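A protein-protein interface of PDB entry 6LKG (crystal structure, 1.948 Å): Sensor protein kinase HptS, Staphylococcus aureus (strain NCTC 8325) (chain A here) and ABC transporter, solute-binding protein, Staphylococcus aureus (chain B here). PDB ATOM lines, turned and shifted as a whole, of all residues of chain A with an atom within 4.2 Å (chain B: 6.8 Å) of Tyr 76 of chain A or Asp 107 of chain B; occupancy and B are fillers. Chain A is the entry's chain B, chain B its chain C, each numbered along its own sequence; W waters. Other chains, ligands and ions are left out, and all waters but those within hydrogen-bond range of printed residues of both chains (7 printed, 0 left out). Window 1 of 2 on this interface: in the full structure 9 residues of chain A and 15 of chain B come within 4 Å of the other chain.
OE1 of Glu 77 of chain A is in hydrogen-bond range of OH of Tyr 200 of chain B (2.6 Å). The side-chain carboxylate (OD2) of Asp 107 of chain B sits at hydrogen-bond distance from the side-chain hydroxyl (OH) of Tyr 76 of chain A, at 2.8 Å. The side-chain carboxylate (OD1) of Asp 107 of chain B is in salt-bridge range of the side-chain amino group (NZ) of Lys 47 of chain A (3.1 Å).
A ring nitrogen (ND1) of His 78 of chain A is in hydrogen-bond range of the backbone carbonyl oxygen (O) of Tyr 76 of chain A. The side-chain amide oxygen (OD1) of Asn 105 of chain B lies within hydrogen-bond range of the backbone NH (N) of Leu 108 of chain B (2.9 Å). N of Ser 106 of chain B lies within hydrogen-bond range of O of Pro 201 of chain B (2.9 Å). The side-chain amide oxygen of Asn 105 of chain B lies within hydrogen-bond range of the backbone NH of Asp 107 of chain B, at 2.8 Å.
Thr 44 of chain A touches Asp 107 of chain B. Thr 44 of chain A touches Gly 110 of chain B (CG2 to CA, 3.8 Å). CD1 of Leu 51 of chain A touches CD2 of Leu 108 of chain B (3.6 Å). Leu 51 of chain A touches Lys 179 of chain B (CD2 to O, 3.8 Å). O of Gly 180 of chain B touches CB of Leu 51 of chain A, at 3.97 Å. CE2 of Tyr 76 of chain A touches O of Ala 178 of chain B, at 3.8 Å. Tyr 76 of chain A touches Lys 198 of chain B. Tyr 76 of chain A touches Gly 199 of chain B. Tyr 200 of chain B touches Tyr 76 of chain A (CD2 to CD2, 3.5 Å). Tyr 76 of chain A touches Pro 201 of chain B.
Of the printed residues of chain B, Thr 44 of chain A touches Asp 107 (3.8 Å) and Gly 110 (3.8 Å). Printed residues of chain B within 4 Å of Leu 51 of chain A: Leu 108 (3.6 Å), Lys 179 (3.8 Å) and Gly 180 (3.97 Å). Asn 74 of chain A touches none of the printed residues of chain B. Tyr 76 of chain A touches six residues of chain B. Printed residues of chain B within 4 Å of Glu 77 of chain A: Lys 198 (3.7 Å) and Tyr 200 (2.6 Å). Printed residues of chain A within 4 Å of Asp 107 of chain B: Thr 44, Lys 47 and Tyr 76. Of the printed residues of chain A, Lys 198 of chain B touches Tyr 76 and Glu 77. The nearest residue of chain B that does not touch Tyr 76 of chain A is Lys 179 of chain B (4.9 Å). The nearest printed residue of chain A that does not touch Asp 107 of chain B is Leu 51 of chain A (4.3 Å).
Of the 9 printed residues of chain A, 5 touch a printed residue of chain B. Hydrophobic or aromatic side chains of chain A that line the printed part of chain B: Leu 51 and Tyr 76. Of the 15 printed residues of chain B, 10 touch a printed residue of chain A. Printed residues of chain B that touch a printed residue of chain A: Asp 107, Leu 108, Gly 110, Ala 178, Lys 179, Gly 180, Lys 198, Gly 199, Tyr 200 and Pro 201. Among the printed residues, 14 pairs touch across the chains.
Water W6 lies within hydrogen-bond range of the side-chain hydroxyl (OG1) of Thr 44 of chain A and the backbone carbonyl oxygen (O) of Asp 107 of chain B. Water W2 lies within hydrogen-bond range of O of Lys 179 of chain B (2.7 Å) and ND2 of Asn 74 of chain A (3.1 Å). Water W5 lies within hydrogen-bond range of the side-chain carboxylate (OD2) of Asp 107 of chain B (2.7 Å) and the side-chain amino group (NZ) of Lys 47 of chain A (3.4 Å). Water W1 bridges O of Tyr 76 of chain A (2.8 Å) and O of Gly 199 of chain B (2.8 Å). Water W7 bridges OE1 of Glu 77 of chain A and NZ of Lys 198 of chain B. Water W4 lies within hydrogen-bond range of the side-chain carboxylate of Asp 107 of chain B (2.8 Å) and the backbone carbonyl oxygen of Thr 73 of chain A (2.9 Å).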
ATOM      1  N   THR A  44     -18.105  15.344   7.350  1.00  0.00           N
ATOM      2  CA  THR A  44     -18.973  14.364   6.705  1.00  0.00           C
ATOM      3  C   THR A  44     -18.466  14.013   5.312  1.00  0.00           C
ATOM      4  O   THR A  44     -18.425  12.835   4.936  1.00  0.00           O
ATOM      5  CB  THR A  44     -20.407  14.891   6.627  1.00  0.00           C
ATOM      6  OG1 THR A  44     -20.922  15.082   7.950  1.00  0.00           O
ATOM      7  CG2 THR A  44     -21.299  13.905   5.879  1.00  0.00           C
ATOM      8  N   LYS A  47     -15.463  11.755   5.775  1.00  0.00           N
ATOM      9  CA  LYS A  47     -15.857  10.412   6.191  1.00  0.00           C
ATOM     10  C   LYS A  47     -16.452   9.629   5.028  1.00  0.00           C
ATOM     11  O   LYS A  47     -16.208   8.423   4.892  1.00  0.00           O
ATOM     12  CB  LYS A  47     -16.854  10.495   7.348  1.00  0.00           C
ATOM     13  CG  LYS A  47     -16.235  10.874   8.681  1.00  0.00           C
ATOM     14  CD  LYS A  47     -17.297  10.986   9.760  1.00  0.00           C
ATOM     15  CE  LYS A  47     -16.684  11.246  11.124  1.00  0.00           C
ATOM     16  NZ  LYS A  47     -17.725  11.381  12.180  1.00  0.00           N
ATOM     17  N   LEU A  51     -14.827   6.083   3.935  1.00  0.00           N
ATOM     18  CA  LEU A  51     -15.630   4.867   3.970  1.00  0.00           C
ATOM     19  C   LEU A  51     -15.843   4.289   2.577  1.00  0.00           C
ATOM     20  O   LEU A  51     -15.908   3.064   2.422  1.00  0.00           O
ATOM     21  CB  LEU A  51     -16.970   5.146   4.653  1.00  0.00           C
ATOM     22  CG  LEU A  51     -16.875   5.318   6.170  1.00  0.00           C
ATOM     23  CD1 LEU A  51     -18.166   5.880   6.740  1.00  0.00           C
ATOM     24  CD2 LEU A  51     -16.522   3.991   6.835  1.00  0.00           C
ATOM     25  N   THR A  73     -12.376   7.919  12.960  1.00  0.00           N
ATOM     26  CA  THR A  73     -12.057   6.517  12.741  1.00  0.00           C
ATOM     27  C   THR A  73     -13.333   5.728  12.490  1.00  0.00           C
ATOM     28  O   THR A  73     -14.423   6.126  12.911  1.00  0.00           O
ATOM     29  CB  THR A  73     -11.294   5.923  13.935  1.00  0.00           C
ATOM     30  OG1 THR A  73     -10.862   4.593  13.620  1.00  0.00           O
ATOM     31  CG2 THR A  73     -12.176   5.884  15.174  1.00  0.00           C
ATOM     32  N   ASN A  74     -13.186   4.610  11.783  1.00  0.00           N
ATOM     33  CA  ASN A  74     -14.254   3.633  11.627  1.00  0.00           C
ATOM     34  C   ASN A  74     -14.058   2.426  12.533  1.00  0.00           C
ATOM     35  O   ASN A  74     -14.749   1.415  12.368  1.00  0.00           O
ATOM     36  CB  ASN A  74     -14.353   3.183  10.169  1.00  0.00           C
ATOM     37  CG  ASN A  74     -13.119   2.431   9.711  1.00  0.00           C
ATOM     38  OD1 ASN A  74     -12.013   2.700  10.174  1.00  0.00           O
ATOM     39  ND2 ASN A  74     -13.303   1.486   8.795  1.00  0.00           N
ATOM     40  N   ASN A  75     -13.122   2.508  13.481  1.00  0.00           N
ATOM     41  CA  ASN A  75     -12.910   1.462  14.479  1.00  0.00           C
ATOM     42  C   ASN A  75     -13.900   1.688  15.624  1.00  0.00           C
ATOM     43  O   ASN A  75     -13.542   2.017  16.758  1.00  0.00           O
ATOM     44  CB  ASN A  75     -11.463   1.472  14.957  1.00  0.00           C
ATOM     45  CG  ASN A  75     -11.156   0.348  15.929  1.00  0.00           C
ATOM     46  OD1 ASN A  75     -11.890  -0.635  16.015  1.00  0.00           O
ATOM     47  ND2 ASN A  75     -10.057   0.489  16.665  1.00  0.00           N
ATOM     48  N   TYR A  76     -15.181   1.504  15.294  1.00  0.00           N
ATOM     49  CA  TYR A  76     -16.250   1.875  16.215  1.00  0.00           C
ATOM     50  C   TYR A  76     -16.255   1.011  17.469  1.00  0.00           C
ATOM     51  O   TYR A  76     -16.701   1.468  18.527  1.00  0.00           O
ATOM     52  CB  TYR A  76     -17.601   1.789  15.506  1.00  0.00           C
ATOM     53  CG  TYR A  76     -17.673   2.603  14.236  1.00  0.00           C
ATOM     54  CD1 TYR A  76     -17.638   3.992  14.278  1.00  0.00           C
ATOM     55  CD2 TYR A  76     -17.774   1.988  12.996  1.00  0.00           C
ATOM     56  CE1 TYR A  76     -17.704   4.745  13.120  1.00  0.00           C
ATOM     57  CE2 TYR A  76     -17.841   2.732  11.831  1.00  0.00           C
ATOM     58  CZ  TYR A  76     -17.806   4.110  11.899  1.00  0.00           C
ATOM     59  OH  TYR A  76     -17.873   4.854  10.745  1.00  0.00           O
ATOM     60  N   GLU A  77     -15.768  -0.222  17.379  1.00  0.00           N
ATOM     61  CA  GLU A  77     -15.694  -1.098  18.539  1.00  0.00           C
ATOM     62  C   GLU A  77     -14.403  -0.920  19.327  1.00  0.00           C
ATOM     63  O   GLU A  77     -14.199  -1.625  20.321  1.00  0.00           O
ATOM     64  CB  GLU A  77     -15.852  -2.559  18.106  1.00  0.00           C
ATOM     65  CG  GLU A  77     -17.212  -2.856  17.482  1.00  0.00           C
ATOM     66  CD  GLU A  77     -17.493  -4.339  17.354  1.00  0.00           C
ATOM     67  OE1 GLU A  77     -17.684  -4.817  16.215  1.00  0.00           O
ATOM     68  OE2 GLU A  77     -17.535  -5.025  18.396  1.00  0.00           O
ATOM     69  N   HIS A  78     -13.544   0.011  18.913  1.00  0.00           N
ATOM     70  CA  HIS A  78     -12.296   0.316  19.613  1.00  0.00           C
ATOM     71  C   HIS A  78     -11.428  -0.930  19.780  1.00  0.00           C
ATOM     72  O   HIS A  78     -10.890  -1.202  20.855  1.00  0.00           O
ATOM     73  CB  HIS A  78     -12.572   0.981  20.963  1.00  0.00           C
ATOM     74  CG  HIS A  78     -13.273   2.298  20.851  1.00  0.00           C
ATOM     75  ND1 HIS A  78     -14.634   2.433  21.017  1.00  0.00           N
ATOM     76  CD2 HIS A  78     -12.804   3.537  20.569  1.00  0.00           C
ATOM     77  CE1 HIS A  78     -14.973   3.699  20.854  1.00  0.00           C
ATOM     78  NE2 HIS A  78     -13.881   4.389  20.579  1.00  0.00           N
ATOM     79  N   VAL B 104     -30.028   4.280   9.621  1.00  0.00           N
ATOM     80  CA  VAL B 104     -29.298   5.319   8.909  1.00  0.00           C
ATOM     81  C   VAL B 104     -27.895   5.402   9.485  1.00  0.00           C
ATOM     82  O   VAL B 104     -27.712   5.381  10.708  1.00  0.00           O
ATOM     83  CB  VAL B 104     -30.005   6.688   9.001  1.00  0.00           C
ATOM     84  CG1 VAL B 104     -29.222   7.745   8.229  1.00  0.00           C
ATOM     85  CG2 VAL B 104     -31.432   6.587   8.487  1.00  0.00           C
ATOM     86  N   ASN B 105     -26.904   5.484   8.602  1.00  0.00           N
ATOM     87  CA  ASN B 105     -25.521   5.679   9.018  1.00  0.00           C
ATOM     88  C   ASN B 105     -25.315   7.162   9.311  1.00  0.00           C
ATOM     89  O   ASN B 105     -25.381   7.998   8.404  1.00  0.00           O
ATOM     90  CB  ASN B 105     -24.562   5.185   7.939  1.00  0.00           C
ATOM     91  CG  ASN B 105     -23.115   5.230   8.382  1.00  0.00           C
ATOM     92  OD1 ASN B 105     -22.577   6.299   8.667  1.00  0.00           O
ATOM     93  ND2 ASN B 105     -22.474   4.069   8.443  1.00  0.00           N
ATOM     94  N   SER B 106     -25.069   7.491  10.582  1.00  0.00           N
ATOM     95  CA  SER B 106     -24.931   8.887  10.975  1.00  0.00           C
ATOM     96  C   SER B 106     -23.597   9.489  10.552  1.00  0.00           C
ATOM     97  O   SER B 106     -23.473  10.719  10.526  1.00  0.00           O
ATOM     98  CB  SER B 106     -25.109   9.034  12.488  1.00  0.00           C
ATOM     99  OG  SER B 106     -24.229   8.179  13.193  1.00  0.00           O
ATOM    100  N   ASP B 107     -22.602   8.662  10.220  1.00  0.00           N
ATOM    101  CA  ASP B 107     -21.359   9.199   9.679  1.00  0.00           C
ATOM    102  C   ASP B 107     -21.532   9.650   8.235  1.00  0.00           C
ATOM    103  O   ASP B 107     -20.878  10.606   7.802  1.00  0.00           O
ATOM    104  CB  ASP B 107     -20.241   8.157   9.769  1.00  0.00           C
ATOM    105  CG  ASP B 107     -19.426   8.277  11.044  1.00  0.00           C
ATOM    106  OD1 ASP B 107     -19.779   9.109  11.906  1.00  0.00           O
ATOM    107  OD2 ASP B 107     -18.427   7.537  11.180  1.00  0.00           O
ATOM    108  N   LEU B 108     -22.411   8.987   7.482  1.00  0.00           N
ATOM    109  CA  LEU B 108     -22.614   9.293   6.073  1.00  0.00           C
ATOM    110  C   LEU B 108     -23.785  10.230   5.813  1.00  0.00           C
ATOM    111  O   LEU B 108     -23.824  10.859   4.749  1.00  0.00           O
ATOM    112  CB  LEU B 108     -22.842   8.000   5.279  1.00  0.00           C
ATOM    113  CG  LEU B 108     -21.714   6.966   5.282  1.00  0.00           C
ATOM    114  CD1 LEU B 108     -22.214   5.633   4.741  1.00  0.00           C
ATOM    115  CD2 LEU B 108     -20.530   7.466   4.472  1.00  0.00           C
ATOM    116  N   GLN B 109     -24.726  10.345   6.755  1.00  0.00           N
ATOM    117  CA  GLN B 109     -25.988  11.027   6.473  1.00  0.00           C
ATOM    118  C   GLN B 109     -25.771  12.490   6.108  1.00  0.00           C
ATOM    119  O   GLN B 109     -26.218  12.950   5.050  1.00  0.00           O
ATOM    120  CB  GLN B 109     -26.929  10.910   7.674  1.00  0.00           C
ATOM    121  CG  GLN B 109     -28.267  11.612   7.468  1.00  0.00           C
ATOM    122  CD  GLN B 109     -29.274  11.305   8.563  1.00  0.00           C
ATOM    123  OE1 GLN B 109     -28.910  10.897   9.665  1.00  0.00           O
ATOM    124  NE2 GLN B 109     -30.553  11.504   8.262  1.00  0.00           N
ATOM    125  N   GLY B 110     -25.091  13.237   6.970  1.00  0.00           N
ATOM    126  CA  GLY B 110     -24.916  14.657   6.711  1.00  0.00           C
ATOM    127  C   GLY B 110     -26.251  15.372   6.799  1.00  0.00           C
ATOM    128  O   GLY B 110     -27.004  15.205   7.765  1.00  0.00           O
ATOM    129  N   ALA B 178     -24.047  -0.252   9.206  1.00  0.00           N
ATOM    130  CA  ALA B 178     -23.256   0.153  10.365  1.00  0.00           C
ATOM    131  C   ALA B 178     -21.791   0.353   9.999  1.00  0.00           C
ATOM    132  O   ALA B 178     -21.132   1.261  10.522  1.00  0.00           O
ATOM    133  CB  ALA B 178     -23.387  -0.886  11.478  1.00  0.00           C
ATOM    134  N   LYS B 179     -21.263  -0.479   9.105  1.00  0.00           N
ATOM    135  CA  LYS B 179     -19.861  -0.410   8.715  1.00  0.00           C
ATOM    136  C   LYS B 179     -19.599   0.594   7.598  1.00  0.00           C
ATOM    137  O   LYS B 179     -18.443   0.763   7.196  1.00  0.00           O
ATOM    138  CB  LYS B 179     -19.362  -1.800   8.305  1.00  0.00           C
ATOM    139  CG  LYS B 179     -19.234  -2.762   9.484  1.00  0.00           C
ATOM    140  CD  LYS B 179     -18.696  -4.121   9.064  1.00  0.00           C
ATOM    141  CE  LYS B 179     -18.580  -5.056  10.260  1.00  0.00           C
ATOM    142  NZ  LYS B 179     -18.111  -6.416   9.872  1.00  0.00           N
ATOM    143  N   GLY B 180     -20.633   1.255   7.087  1.00  0.00           N
ATOM    144  CA  GLY B 180     -20.449   2.355   6.162  1.00  0.00           C
ATOM    145  C   GLY B 180     -20.512   2.010   4.693  1.00  0.00           C
ATOM    146  O   GLY B 180     -20.099   2.834   3.867  1.00  0.00           O
ATOM    147  N   LYS B 198     -23.056  -1.574  20.071  1.00  0.00           N
ATOM    148  CA  LYS B 198     -21.637  -1.884  19.950  1.00  0.00           C
ATOM    149  C   LYS B 198     -20.802  -0.670  19.571  1.00  0.00           C
ATOM    150  O   LYS B 198     -19.577  -0.795  19.456  1.00  0.00           O
ATOM    151  CB  LYS B 198     -21.417  -2.996  18.919  1.00  0.00           C
ATOM    152  CG  LYS B 198     -21.877  -4.371  19.373  1.00  0.00           C
ATOM    153  CD  LYS B 198     -21.392  -5.453  18.420  1.00  0.00           C
ATOM    154  CE  LYS B 198     -22.072  -5.347  17.064  1.00  0.00           C
ATOM    155  NZ  LYS B 198     -21.742  -6.504  16.185  1.00  0.00           N
ATOM    156  N   GLY B 199     -21.424   0.492  19.377  1.00  0.00           N
ATOM    157  CA  GLY B 199     -20.711   1.720  19.081  1.00  0.00           C
ATOM    158  C   GLY B 199     -20.796   2.178  17.642  1.00  0.00           C
ATOM    159  O   GLY B 199     -20.205   3.211  17.305  1.00  0.00           O
ATOM    160  N   TYR B 200     -21.509   1.455  16.782  1.00  0.00           N
ATOM    161  CA  TYR B 200     -21.563   1.810  15.375  1.00  0.00           C
ATOM    162  C   TYR B 200     -22.463   3.027  15.156  1.00  0.00           C
ATOM    163  O   TYR B 200     -23.403   3.259  15.922  1.00  0.00           O
ATOM    164  CB  TYR B 200     -22.064   0.627  14.552  1.00  0.00           C
ATOM    165  CG  TYR B 200     -21.026  -0.462  14.419  1.00  0.00           C
ATOM    166  CD1 TYR B 200     -20.885  -1.435  15.399  1.00  0.00           C
ATOM    167  CD2 TYR B 200     -20.174  -0.505  13.324  1.00  0.00           C
ATOM    168  CE1 TYR B 200     -19.930  -2.427  15.287  1.00  0.00           C
ATOM    169  CE2 TYR B 200     -19.218  -1.492  13.203  1.00  0.00           C
ATOM    170  CZ  TYR B 200     -19.100  -2.450  14.186  1.00  0.00           C
ATOM    171  OH  TYR B 200     -18.146  -3.431  14.065  1.00  0.00           O
ATOM    172  N   PRO B 201     -22.182   3.830  14.125  1.00  0.00           N
ATOM    173  CA  PRO B 201     -22.966   5.060  13.884  1.00  0.00           C
ATOM    174  C   PRO B 201     -24.312   4.759  13.236  1.00  0.00           C
ATOM    175  O   PRO B 201     -24.560   5.030  12.059  1.00  0.00           O
ATOM    176  CB  PRO B 201     -22.036   5.864  12.971  1.00  0.00           C
ATOM    177  CG  PRO B 201     -21.326   4.818  12.181  1.00  0.00           C
ATOM    178  CD  PRO B 201     -21.105   3.664  13.130  1.00  0.00           C
ATOM    179  N   VAL B 202     -25.216   4.182  14.023  1.00  0.00           N
ATOM    180  CA  VAL B 202     -26.508   3.714  13.537  1.00  0.00           C
ATOM    181  C   VAL B 202     -27.598   4.557  14.182  1.00  0.00           C
ATOM    182  O   VAL B 202     -27.706   4.608  15.414  1.00  0.00           O
ATOM    183  CB  VAL B 202     -26.721   2.223  13.841  1.00  0.00           C
ATOM    184  CG1 VAL B 202     -28.119   1.788  13.416  1.00  0.00           C
ATOM    185  CG2 VAL B 202     -25.658   1.386  13.153  1.00  0.00           C
HETATM  186  O   HOH W   1     -17.890   3.941  18.779  1.00  0.00           O
HETATM  187  O   HOH W   2     -16.139   0.220   8.460  1.00  0.00           O
HETATM  188  O   HOH W   3     -19.741   3.300   9.164  1.00  0.00           O
HETATM  189  O   HOH W   4     -15.638   7.790  10.809  1.00  0.00           O
HETATM  190  O   HOH W   5     -17.593   8.360  13.628  1.00  0.00           O
HETATM  191  O   HOH W   6     -20.934  12.944   9.339  1.00  0.00           O
HETATM  192  O   HOH W   7     -19.026  -7.257  15.895  1.00  0.00           O
